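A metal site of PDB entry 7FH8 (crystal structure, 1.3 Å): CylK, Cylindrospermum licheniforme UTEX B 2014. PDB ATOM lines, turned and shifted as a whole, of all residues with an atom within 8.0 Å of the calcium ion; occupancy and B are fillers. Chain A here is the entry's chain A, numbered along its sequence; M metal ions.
OE2 of Glu 167 binds the calcium ion, at 2.3 Å.
O of Tyr 165 is bound to the calcium ion, 2.3 Å away.
The calcium ion is bound by O of Leu 220 (2.3 Å).
OD1 of Asp 219 is bound to the calcium ion (2.3 Å).
The calcium ion is bound by O of Gln 176 (2.3 Å).
The calcium ion is bound by O of Gly 173.
The backbone NH (N) of Leu 174 lies within hydrogen-bond range of the side-chain carboxylate (OE1) of Glu 167, 3.5 Å away.
The backbone NH of Asn 175 is in hydrogen-bond range of the side-chain carboxylate of Glu 167 (2.9 Å).
O of Leu 172 lies within hydrogen-bond range of N of Leu 220, 2.9 Å away.
The backbone NH (N) of Asp 168 is in hydrogen-bond range of the side-chain carboxylate (OD2) of Asp 219 (3.1 Å).
The backbone carbonyl oxygen (O) of Asp 219 sits at hydrogen-bond distance from the backbone NH (N) of Trp 212 (2.8 Å).
The side-chain hydroxyl (OG1) of Thr 171 lies within hydrogen-bond range of the backbone NH (N) of Gly 173, 3.0 Å away.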
ATOM      1  N   PHE A 114       6.906   3.171 -14.280  1.00  0.00           N
ATOM      2  CA  PHE A 114       5.919   2.890 -13.241  1.00  0.00           C
ATOM      3  C   PHE A 114       6.579   1.979 -12.213  1.00  0.00           C
ATOM      4  O   PHE A 114       7.068   0.898 -12.573  1.00  0.00           O
ATOM      5  CB  PHE A 114       4.720   2.194 -13.886  1.00  0.00           C
ATOM      6  CG  PHE A 114       3.591   1.868 -12.937  1.00  0.00           C
ATOM      7  CD1 PHE A 114       3.567   0.673 -12.236  1.00  0.00           C
ATOM      8  CD2 PHE A 114       2.507   2.740 -12.824  1.00  0.00           C
ATOM      9  CE1 PHE A 114       2.505   0.366 -11.390  1.00  0.00           C
ATOM     10  CE2 PHE A 114       1.438   2.436 -11.984  1.00  0.00           C
ATOM     11  CZ  PHE A 114       1.437   1.253 -11.259  1.00  0.00           C
ATOM     12  N   ARG A 125      -1.894   8.261 -13.430  1.00  0.00           N
ATOM     13  CA  ARG A 125      -0.544   7.964 -13.906  1.00  0.00           C
ATOM     14  C   ARG A 125      -0.556   7.703 -15.407  1.00  0.00           C
ATOM     15  O   ARG A 125      -1.112   6.706 -15.862  1.00  0.00           O
ATOM     16  CB  ARG A 125       0.069   6.782 -13.153  1.00  0.00           C
ATOM     17  CG  ARG A 125       0.438   7.097 -11.712  1.00  0.00           C
ATOM     18  CD  ARG A 125       1.654   8.020 -11.687  1.00  0.00           C
ATOM     19  NE  ARG A 125       2.884   7.280 -11.959  1.00  0.00           N
ATOM     20  CZ  ARG A 125       3.488   7.230 -13.134  1.00  0.00           C
ATOM     21  NH1 ARG A 125       3.080   7.944 -14.170  1.00  0.00           N
ATOM     22  NH2 ARG A 125       4.554   6.428 -13.277  1.00  0.00           N
ATOM     23  N   TYR A 164       1.638  -3.444 -14.908  1.00  0.00           N
ATOM     24  CA  TYR A 164       1.776  -2.070 -14.451  1.00  0.00           C
ATOM     25  C   TYR A 164       0.528  -1.292 -14.869  1.00  0.00           C
ATOM     26  O   TYR A 164      -0.259  -1.742 -15.711  1.00  0.00           O
ATOM     27  CB  TYR A 164       3.036  -1.427 -15.051  1.00  0.00           C
ATOM     28  CG  TYR A 164       4.370  -2.002 -14.579  1.00  0.00           C
ATOM     29  CD1 TYR A 164       4.438  -3.056 -13.663  1.00  0.00           C
ATOM     30  CD2 TYR A 164       5.564  -1.476 -15.051  1.00  0.00           C
ATOM     31  CE1 TYR A 164       5.674  -3.565 -13.246  1.00  0.00           C
ATOM     32  CE2 TYR A 164       6.780  -1.979 -14.654  1.00  0.00           C
ATOM     33  CZ  TYR A 164       6.842  -3.018 -13.758  1.00  0.00           C
ATOM     34  OH  TYR A 164       8.084  -3.491 -13.377  1.00  0.00           O
ATOM     35  N   TYR A 165       0.346  -0.104 -14.274  1.00  0.00           N
ATOM     36  CA  TYR A 165      -0.781   0.768 -14.623  1.00  0.00           C
ATOM     37  C   TYR A 165      -2.119   0.089 -14.376  1.00  0.00           C
ATOM     38  O   TYR A 165      -3.099   0.340 -15.087  1.00  0.00           O
ATOM     39  CB  TYR A 165      -0.703   1.294 -16.070  1.00  0.00           C
ATOM     40  CG  TYR A 165       0.652   1.846 -16.419  1.00  0.00           C
ATOM     41  CD1 TYR A 165       1.033   3.129 -16.044  1.00  0.00           C
ATOM     42  CD2 TYR A 165       1.575   1.064 -17.109  1.00  0.00           C
ATOM     43  CE1 TYR A 165       2.309   3.622 -16.348  1.00  0.00           C
ATOM     44  CE2 TYR A 165       2.834   1.539 -17.416  1.00  0.00           C
ATOM     45  CZ  TYR A 165       3.200   2.812 -17.030  1.00  0.00           C
ATOM     46  OH  TYR A 165       4.463   3.266 -17.334  1.00  0.00           O
ATOM     47  N   PHE A 166      -2.181  -0.778 -13.372  1.00  0.00           N
ATOM     48  CA  PHE A 166      -3.296  -1.695 -13.178  1.00  0.00           C
ATOM     49  C   PHE A 166      -4.081  -1.260 -11.944  1.00  0.00           C
ATOM     50  O   PHE A 166      -3.576  -1.345 -10.826  1.00  0.00           O
ATOM     51  CB  PHE A 166      -2.745  -3.112 -13.044  1.00  0.00           C
ATOM     52  CG  PHE A 166      -3.785  -4.160 -12.808  1.00  0.00           C
ATOM     53  CD1 PHE A 166      -4.882  -4.280 -13.640  1.00  0.00           C
ATOM     54  CD2 PHE A 166      -3.627  -5.083 -11.780  1.00  0.00           C
ATOM     55  CE1 PHE A 166      -5.828  -5.274 -13.435  1.00  0.00           C
ATOM     56  CE2 PHE A 166      -4.558  -6.071 -11.560  1.00  0.00           C
ATOM     57  CZ  PHE A 166      -5.659  -6.170 -12.395  1.00  0.00           C
ATOM     58  N   GLU A 167      -5.306  -0.778 -12.165  1.00  0.00           N
ATOM     59  CA  GLU A 167      -6.128  -0.292 -11.067  1.00  0.00           C
ATOM     60  C   GLU A 167      -6.986  -1.379 -10.431  1.00  0.00           C
ATOM     61  O   GLU A 167      -7.384  -1.232  -9.270  1.00  0.00           O
ATOM     62  CB  GLU A 167      -7.014   0.874 -11.528  1.00  0.00           C
ATOM     63  CG  GLU A 167      -6.201   2.093 -11.961  1.00  0.00           C
ATOM     64  CD  GLU A 167      -6.503   2.506 -13.388  1.00  0.00           C
ATOM     65  OE1 GLU A 167      -7.505   3.203 -13.614  1.00  0.00           O
ATOM     66  OE2 GLU A 167      -5.731   2.123 -14.289  1.00  0.00           O
ATOM     67  N   ASP A 168      -7.282  -2.452 -11.167  1.00  0.00           N
ATOM     68  CA  ASP A 168      -7.953  -3.624 -10.600  1.00  0.00           C
ATOM     69  C   ASP A 168      -9.276  -3.246  -9.922  1.00  0.00           C
ATOM     70  O   ASP A 168      -9.538  -3.599  -8.770  1.00  0.00           O
ATOM     71  CB  ASP A 168      -7.021  -4.376  -9.645  1.00  0.00           C
ATOM     72  CG  ASP A 168      -7.490  -5.787  -9.326  1.00  0.00           C
ATOM     73  OD1 ASP A 168      -8.471  -6.250  -9.952  1.00  0.00           O
ATOM     74  OD2 ASP A 168      -6.872  -6.430  -8.444  1.00  0.00           O
ATOM     75  N   ASP A 169     -10.093  -2.492 -10.644  1.00  0.00           N
ATOM     76  CA  ASP A 169     -11.363  -2.036 -10.094  1.00  0.00           C
ATOM     77  C   ASP A 169     -12.514  -2.235 -11.071  1.00  0.00           C
ATOM     78  O   ASP A 169     -12.354  -2.908 -12.097  1.00  0.00           O
ATOM     79  CB  ASP A 169     -11.264  -0.583  -9.587  1.00  0.00           C
ATOM     80  CG  ASP A 169     -10.954   0.422 -10.690  1.00  0.00           C
ATOM     81  OD1 ASP A 169     -11.170   0.121 -11.886  1.00  0.00           O
ATOM     82  OD2 ASP A 169     -10.476   1.524 -10.354  1.00  0.00           O
ATOM     83  N   THR A 171     -13.902  -0.193 -13.087  1.00  0.00           N
ATOM     84  CA  THR A 171     -13.852   0.639 -14.278  1.00  0.00           C
ATOM     85  C   THR A 171     -13.021  -0.036 -15.360  1.00  0.00           C
ATOM     86  O   THR A 171     -12.514  -1.154 -15.202  1.00  0.00           O
ATOM     87  CB  THR A 171     -13.258   2.015 -13.954  1.00  0.00           C
ATOM     88  OG1 THR A 171     -11.831   1.902 -13.826  1.00  0.00           O
ATOM     89  CG2 THR A 171     -13.822   2.548 -12.646  1.00  0.00           C
ATOM     90  N   LEU A 172     -12.862   0.656 -16.488  1.00  0.00           N
ATOM     91  CA  LEU A 172     -11.981   0.186 -17.553  1.00  0.00           C
ATOM     92  C   LEU A 172     -10.510   0.438 -17.264  1.00  0.00           C
ATOM     93  O   LEU A 172      -9.661   0.138 -18.112  1.00  0.00           O
ATOM     94  CB  LEU A 172     -12.372   0.830 -18.890  1.00  0.00           C
ATOM     95  CG  LEU A 172     -13.641   0.298 -19.585  1.00  0.00           C
ATOM     96  CD1 LEU A 172     -13.836   1.014 -20.904  1.00  0.00           C
ATOM     97  CD2 LEU A 172     -13.560  -1.205 -19.795  1.00  0.00           C
ATOM     98  N   GLY A 173     -10.173   0.983 -16.091  1.00  0.00           N
ATOM     99  CA  GLY A 173      -8.788   1.182 -15.735  1.00  0.00           C
ATOM    100  C   GLY A 173      -8.106   2.231 -16.583  1.00  0.00           C
ATOM    101  O   GLY A 173      -6.973   2.021 -17.033  1.00  0.00           O
ATOM    102  N   LEU A 174      -8.777   3.356 -16.823  1.00  0.00           N
ATOM    103  CA  LEU A 174      -8.250   4.424 -17.658  1.00  0.00           C
ATOM    104  C   LEU A 174      -7.433   5.446 -16.875  1.00  0.00           C
ATOM    105  O   LEU A 174      -6.778   6.303 -17.501  1.00  0.00           O
ATOM    106  CB  LEU A 174      -9.405   5.159 -18.355  1.00  0.00           C
ATOM    107  CG  LEU A 174     -10.409   4.279 -19.094  1.00  0.00           C
ATOM    108  CD1 LEU A 174     -11.448   5.127 -19.826  1.00  0.00           C
ATOM    109  CD2 LEU A 174      -9.690   3.361 -20.059  1.00  0.00           C
ATOM    110  N   ASN A 175      -7.444   5.393 -15.541  1.00  0.00           N
ATOM    111  CA  ASN A 175      -6.779   6.403 -14.743  1.00  0.00           C
ATOM    112  C   ASN A 175      -5.261   6.232 -14.753  1.00  0.00           C
ATOM    113  O   ASN A 175      -4.531   7.202 -14.507  1.00  0.00           O
ATOM    114  CB  ASN A 175      -7.286   6.328 -13.301  1.00  0.00           C
ATOM    115  CG  ASN A 175      -7.252   7.670 -12.594  1.00  0.00           C
ATOM    116  OD1 ASN A 175      -7.457   8.710 -13.220  1.00  0.00           O
ATOM    117  ND2 ASN A 175      -7.001   7.658 -11.288  1.00  0.00           N
ATOM    118  N   GLN A 176      -4.774   5.027 -15.049  1.00  0.00           N
ATOM    119  CA  GLN A 176      -3.350   4.746 -15.175  1.00  0.00           C
ATOM    120  C   GLN A 176      -3.125   3.981 -16.468  1.00  0.00           C
ATOM    121  O   GLN A 176      -3.815   2.988 -16.731  1.00  0.00           O
ATOM    122  CB  GLN A 176      -2.851   3.911 -13.993  1.00  0.00           C
ATOM    123  CG  GLN A 176      -3.067   4.584 -12.652  1.00  0.00           C
ATOM    124  CD  GLN A 176      -2.446   3.801 -11.516  1.00  0.00           C
ATOM    125  OE1 GLN A 176      -2.061   2.635 -11.670  1.00  0.00           O
ATOM    126  NE2 GLN A 176      -2.332   4.440 -10.353  1.00  0.00           N
ATOM    127  N   SER A 177      -2.164   4.426 -17.269  1.00  0.00           N
ATOM    128  CA  SER A 177      -1.887   3.784 -18.546  1.00  0.00           C
ATOM    129  C   SER A 177      -0.572   4.304 -19.081  1.00  0.00           C
ATOM    130  O   SER A 177      -0.188   5.455 -18.825  1.00  0.00           O
ATOM    131  CB  SER A 177      -3.005   4.071 -19.569  1.00  0.00           C
ATOM    132  OG  SER A 177      -2.774   3.405 -20.794  1.00  0.00           O
ATOM    133  N   ALA A 178       0.108   3.469 -19.851  1.00  0.00           N
ATOM    134  CA  ALA A 178       1.233   3.910 -20.643  1.00  0.00           C
ATOM    135  C   ALA A 178       0.717   4.380 -21.999  1.00  0.00           C
ATOM    136  O   ALA A 178      -0.332   3.938 -22.465  1.00  0.00           O
ATOM    137  CB  ALA A 178       2.219   2.755 -20.868  1.00  0.00           C
ATOM    138  N   ILE A 210      -4.102  -1.793 -25.332  1.00  0.00           N
ATOM    139  CA  ILE A 210      -3.764  -3.059 -24.694  1.00  0.00           C
ATOM    140  C   ILE A 210      -4.529  -3.134 -23.388  1.00  0.00           C
ATOM    141  O   ILE A 210      -4.223  -2.399 -22.441  1.00  0.00           O
ATOM    142  CB  ILE A 210      -2.260  -3.180 -24.415  1.00  0.00           C
ATOM    143  CG1 ILE A 210      -1.422  -2.989 -25.683  1.00  0.00           C
ATOM    144  CG2 ILE A 210      -1.970  -4.528 -23.742  1.00  0.00           C
ATOM    145  CD1 ILE A 210       0.066  -2.822 -25.395  1.00  0.00           C
ATOM    146  N   PHE A 211      -5.525  -4.023 -23.316  1.00  0.00           N
ATOM    147  CA  PHE A 211      -6.294  -4.233 -22.107  1.00  0.00           C
ATOM    148  C   PHE A 211      -5.874  -5.521 -21.414  1.00  0.00           C
ATOM    149  O   PHE A 211      -5.782  -6.576 -22.051  1.00  0.00           O
ATOM    150  CB  PHE A 211      -7.791  -4.306 -22.400  1.00  0.00           C
ATOM    151  CG  PHE A 211      -8.452  -2.967 -22.580  1.00  0.00           C
ATOM    152  CD1 PHE A 211      -8.893  -2.260 -21.468  1.00  0.00           C
ATOM    153  CD2 PHE A 211      -8.652  -2.436 -23.839  1.00  0.00           C
ATOM    154  CE1 PHE A 211      -9.519  -1.025 -21.615  1.00  0.00           C
ATOM    155  CE2 PHE A 211      -9.272  -1.210 -23.995  1.00  0.00           C
ATOM    156  CZ  PHE A 211      -9.706  -0.503 -22.890  1.00  0.00           C
ATOM    157  N   TRP A 212      -5.653  -5.438 -20.106  1.00  0.00           N
ATOM    158  CA  TRP A 212      -5.633  -6.633 -19.275  1.00  0.00           C
ATOM    159  C   TRP A 212      -7.078  -7.111 -19.145  1.00  0.00           C
ATOM    160  O   TRP A 212      -7.993  -6.310 -18.947  1.00  0.00           O
ATOM    161  CB  TRP A 212      -5.089  -6.292 -17.884  1.00  0.00           C
ATOM    162  CG  TRP A 212      -5.218  -7.423 -16.901  1.00  0.00           C
ATOM    163  CD1 TRP A 212      -6.266  -7.681 -16.052  1.00  0.00           C
ATOM    164  CD2 TRP A 212      -4.256  -8.457 -16.658  1.00  0.00           C
ATOM    165  NE1 TRP A 212      -6.015  -8.800 -15.310  1.00  0.00           N
ATOM    166  CE2 TRP A 212      -4.779  -9.300 -15.653  1.00  0.00           C
ATOM    167  CE3 TRP A 212      -2.999  -8.752 -17.186  1.00  0.00           C
ATOM    168  CZ2 TRP A 212      -4.093 -10.420 -15.181  1.00  0.00           C
ATOM    169  CZ3 TRP A 212      -2.312  -9.862 -16.712  1.00  0.00           C
ATOM    170  CH2 TRP A 212      -2.860 -10.679 -15.717  1.00  0.00           C
ATOM    171  N   TYR A 218     -11.973  -5.539 -17.483  1.00  0.00           N
ATOM    172  CA  TYR A 218     -10.827  -5.046 -18.236  1.00  0.00           C
ATOM    173  C   TYR A 218     -10.110  -3.920 -17.494  1.00  0.00           C
ATOM    174  O   TYR A 218     -10.700  -3.206 -16.694  1.00  0.00           O
ATOM    175  CB  TYR A 218     -11.254  -4.505 -19.599  1.00  0.00           C
ATOM    176  CG  TYR A 218     -11.870  -5.517 -20.533  1.00  0.00           C
ATOM    177  CD1 TYR A 218     -11.056  -6.265 -21.377  1.00  0.00           C
ATOM    178  CD2 TYR A 218     -13.239  -5.701 -20.599  1.00  0.00           C
ATOM    179  CE1 TYR A 218     -11.602  -7.185 -22.250  1.00  0.00           C
ATOM    180  CE2 TYR A 218     -13.792  -6.622 -21.464  1.00  0.00           C
ATOM    181  CZ  TYR A 218     -12.969  -7.355 -22.284  1.00  0.00           C
ATOM    182  OH  TYR A 218     -13.514  -8.276 -23.157  1.00  0.00           O
ATOM    183  N   ASP A 219      -8.830  -3.752 -17.821  1.00  0.00           N
ATOM    184  CA  ASP A 219      -8.049  -2.622 -17.315  1.00  0.00           C
ATOM    185  C   ASP A 219      -7.058  -2.212 -18.388  1.00  0.00           C
ATOM    186  O   ASP A 219      -6.246  -3.034 -18.837  1.00  0.00           O
ATOM    187  CB  ASP A 219      -7.327  -2.995 -16.029  1.00  0.00           C
ATOM    188  CG  ASP A 219      -6.769  -1.785 -15.290  1.00  0.00           C
ATOM    189  OD1 ASP A 219      -5.948  -1.061 -15.878  1.00  0.00           O
ATOM    190  OD2 ASP A 219      -7.171  -1.565 -14.130  1.00  0.00           O
ATOM    191  N   LEU A 220      -7.109  -0.946 -18.804  1.00  0.00           N
ATOM    192  CA  LEU A 220      -6.205  -0.442 -19.819  1.00  0.00           C
ATOM    193  C   LEU A 220      -4.775  -0.386 -19.279  1.00  0.00           C
ATOM    194  O   LEU A 220      -4.488   0.317 -18.309  1.00  0.00           O
ATOM    195  CB  LEU A 220      -6.631   0.953 -20.256  1.00  0.00           C
ATOM    196  CG  LEU A 220      -5.739   1.622 -21.321  1.00  0.00           C
ATOM    197  CD1 LEU A 220      -5.829   0.909 -22.662  1.00  0.00           C
ATOM    198  CD2 LEU A 220      -6.103   3.101 -21.489  1.00  0.00           C
ATOM    199  N   ILE A 221      -3.866  -1.122 -19.925  1.00  0.00           N
ATOM    200  CA  ILE A 221      -2.461  -1.092 -19.556  1.00  0.00           C
ATOM    201  C   ILE A 221      -1.685  -0.079 -20.394  1.00  0.00           C
ATOM    202  O   ILE A 221      -0.844   0.659 -19.872  1.00  0.00           O
ATOM    203  CB  ILE A 221      -1.854  -2.506 -19.650  1.00  0.00           C
ATOM    204  CG1 ILE A 221      -2.685  -3.505 -18.839  1.00  0.00           C
ATOM    205  CG2 ILE A 221      -0.368  -2.510 -19.213  1.00  0.00           C
ATOM    206  CD1 ILE A 221      -2.873  -3.135 -17.381  1.00  0.00           C
ATOM    207  N   GLY A 222      -1.952  -0.024 -21.699  1.00  0.00           N
ATOM    208  CA  GLY A 222      -1.193   0.862 -22.561  1.00  0.00           C
ATOM    209  C   GLY A 222      -1.901   1.134 -23.866  1.00  0.00           C
ATOM    210  O   GLY A 222      -2.727   0.342 -24.333  1.00  0.00           O
HETATM  211 CA    CA M   1      -4.994   1.047 -16.173  1.00  0.00          CA
HETATM  212 MG    MG M   2     -11.521  -2.986 -14.501  1.00  0.00          MG
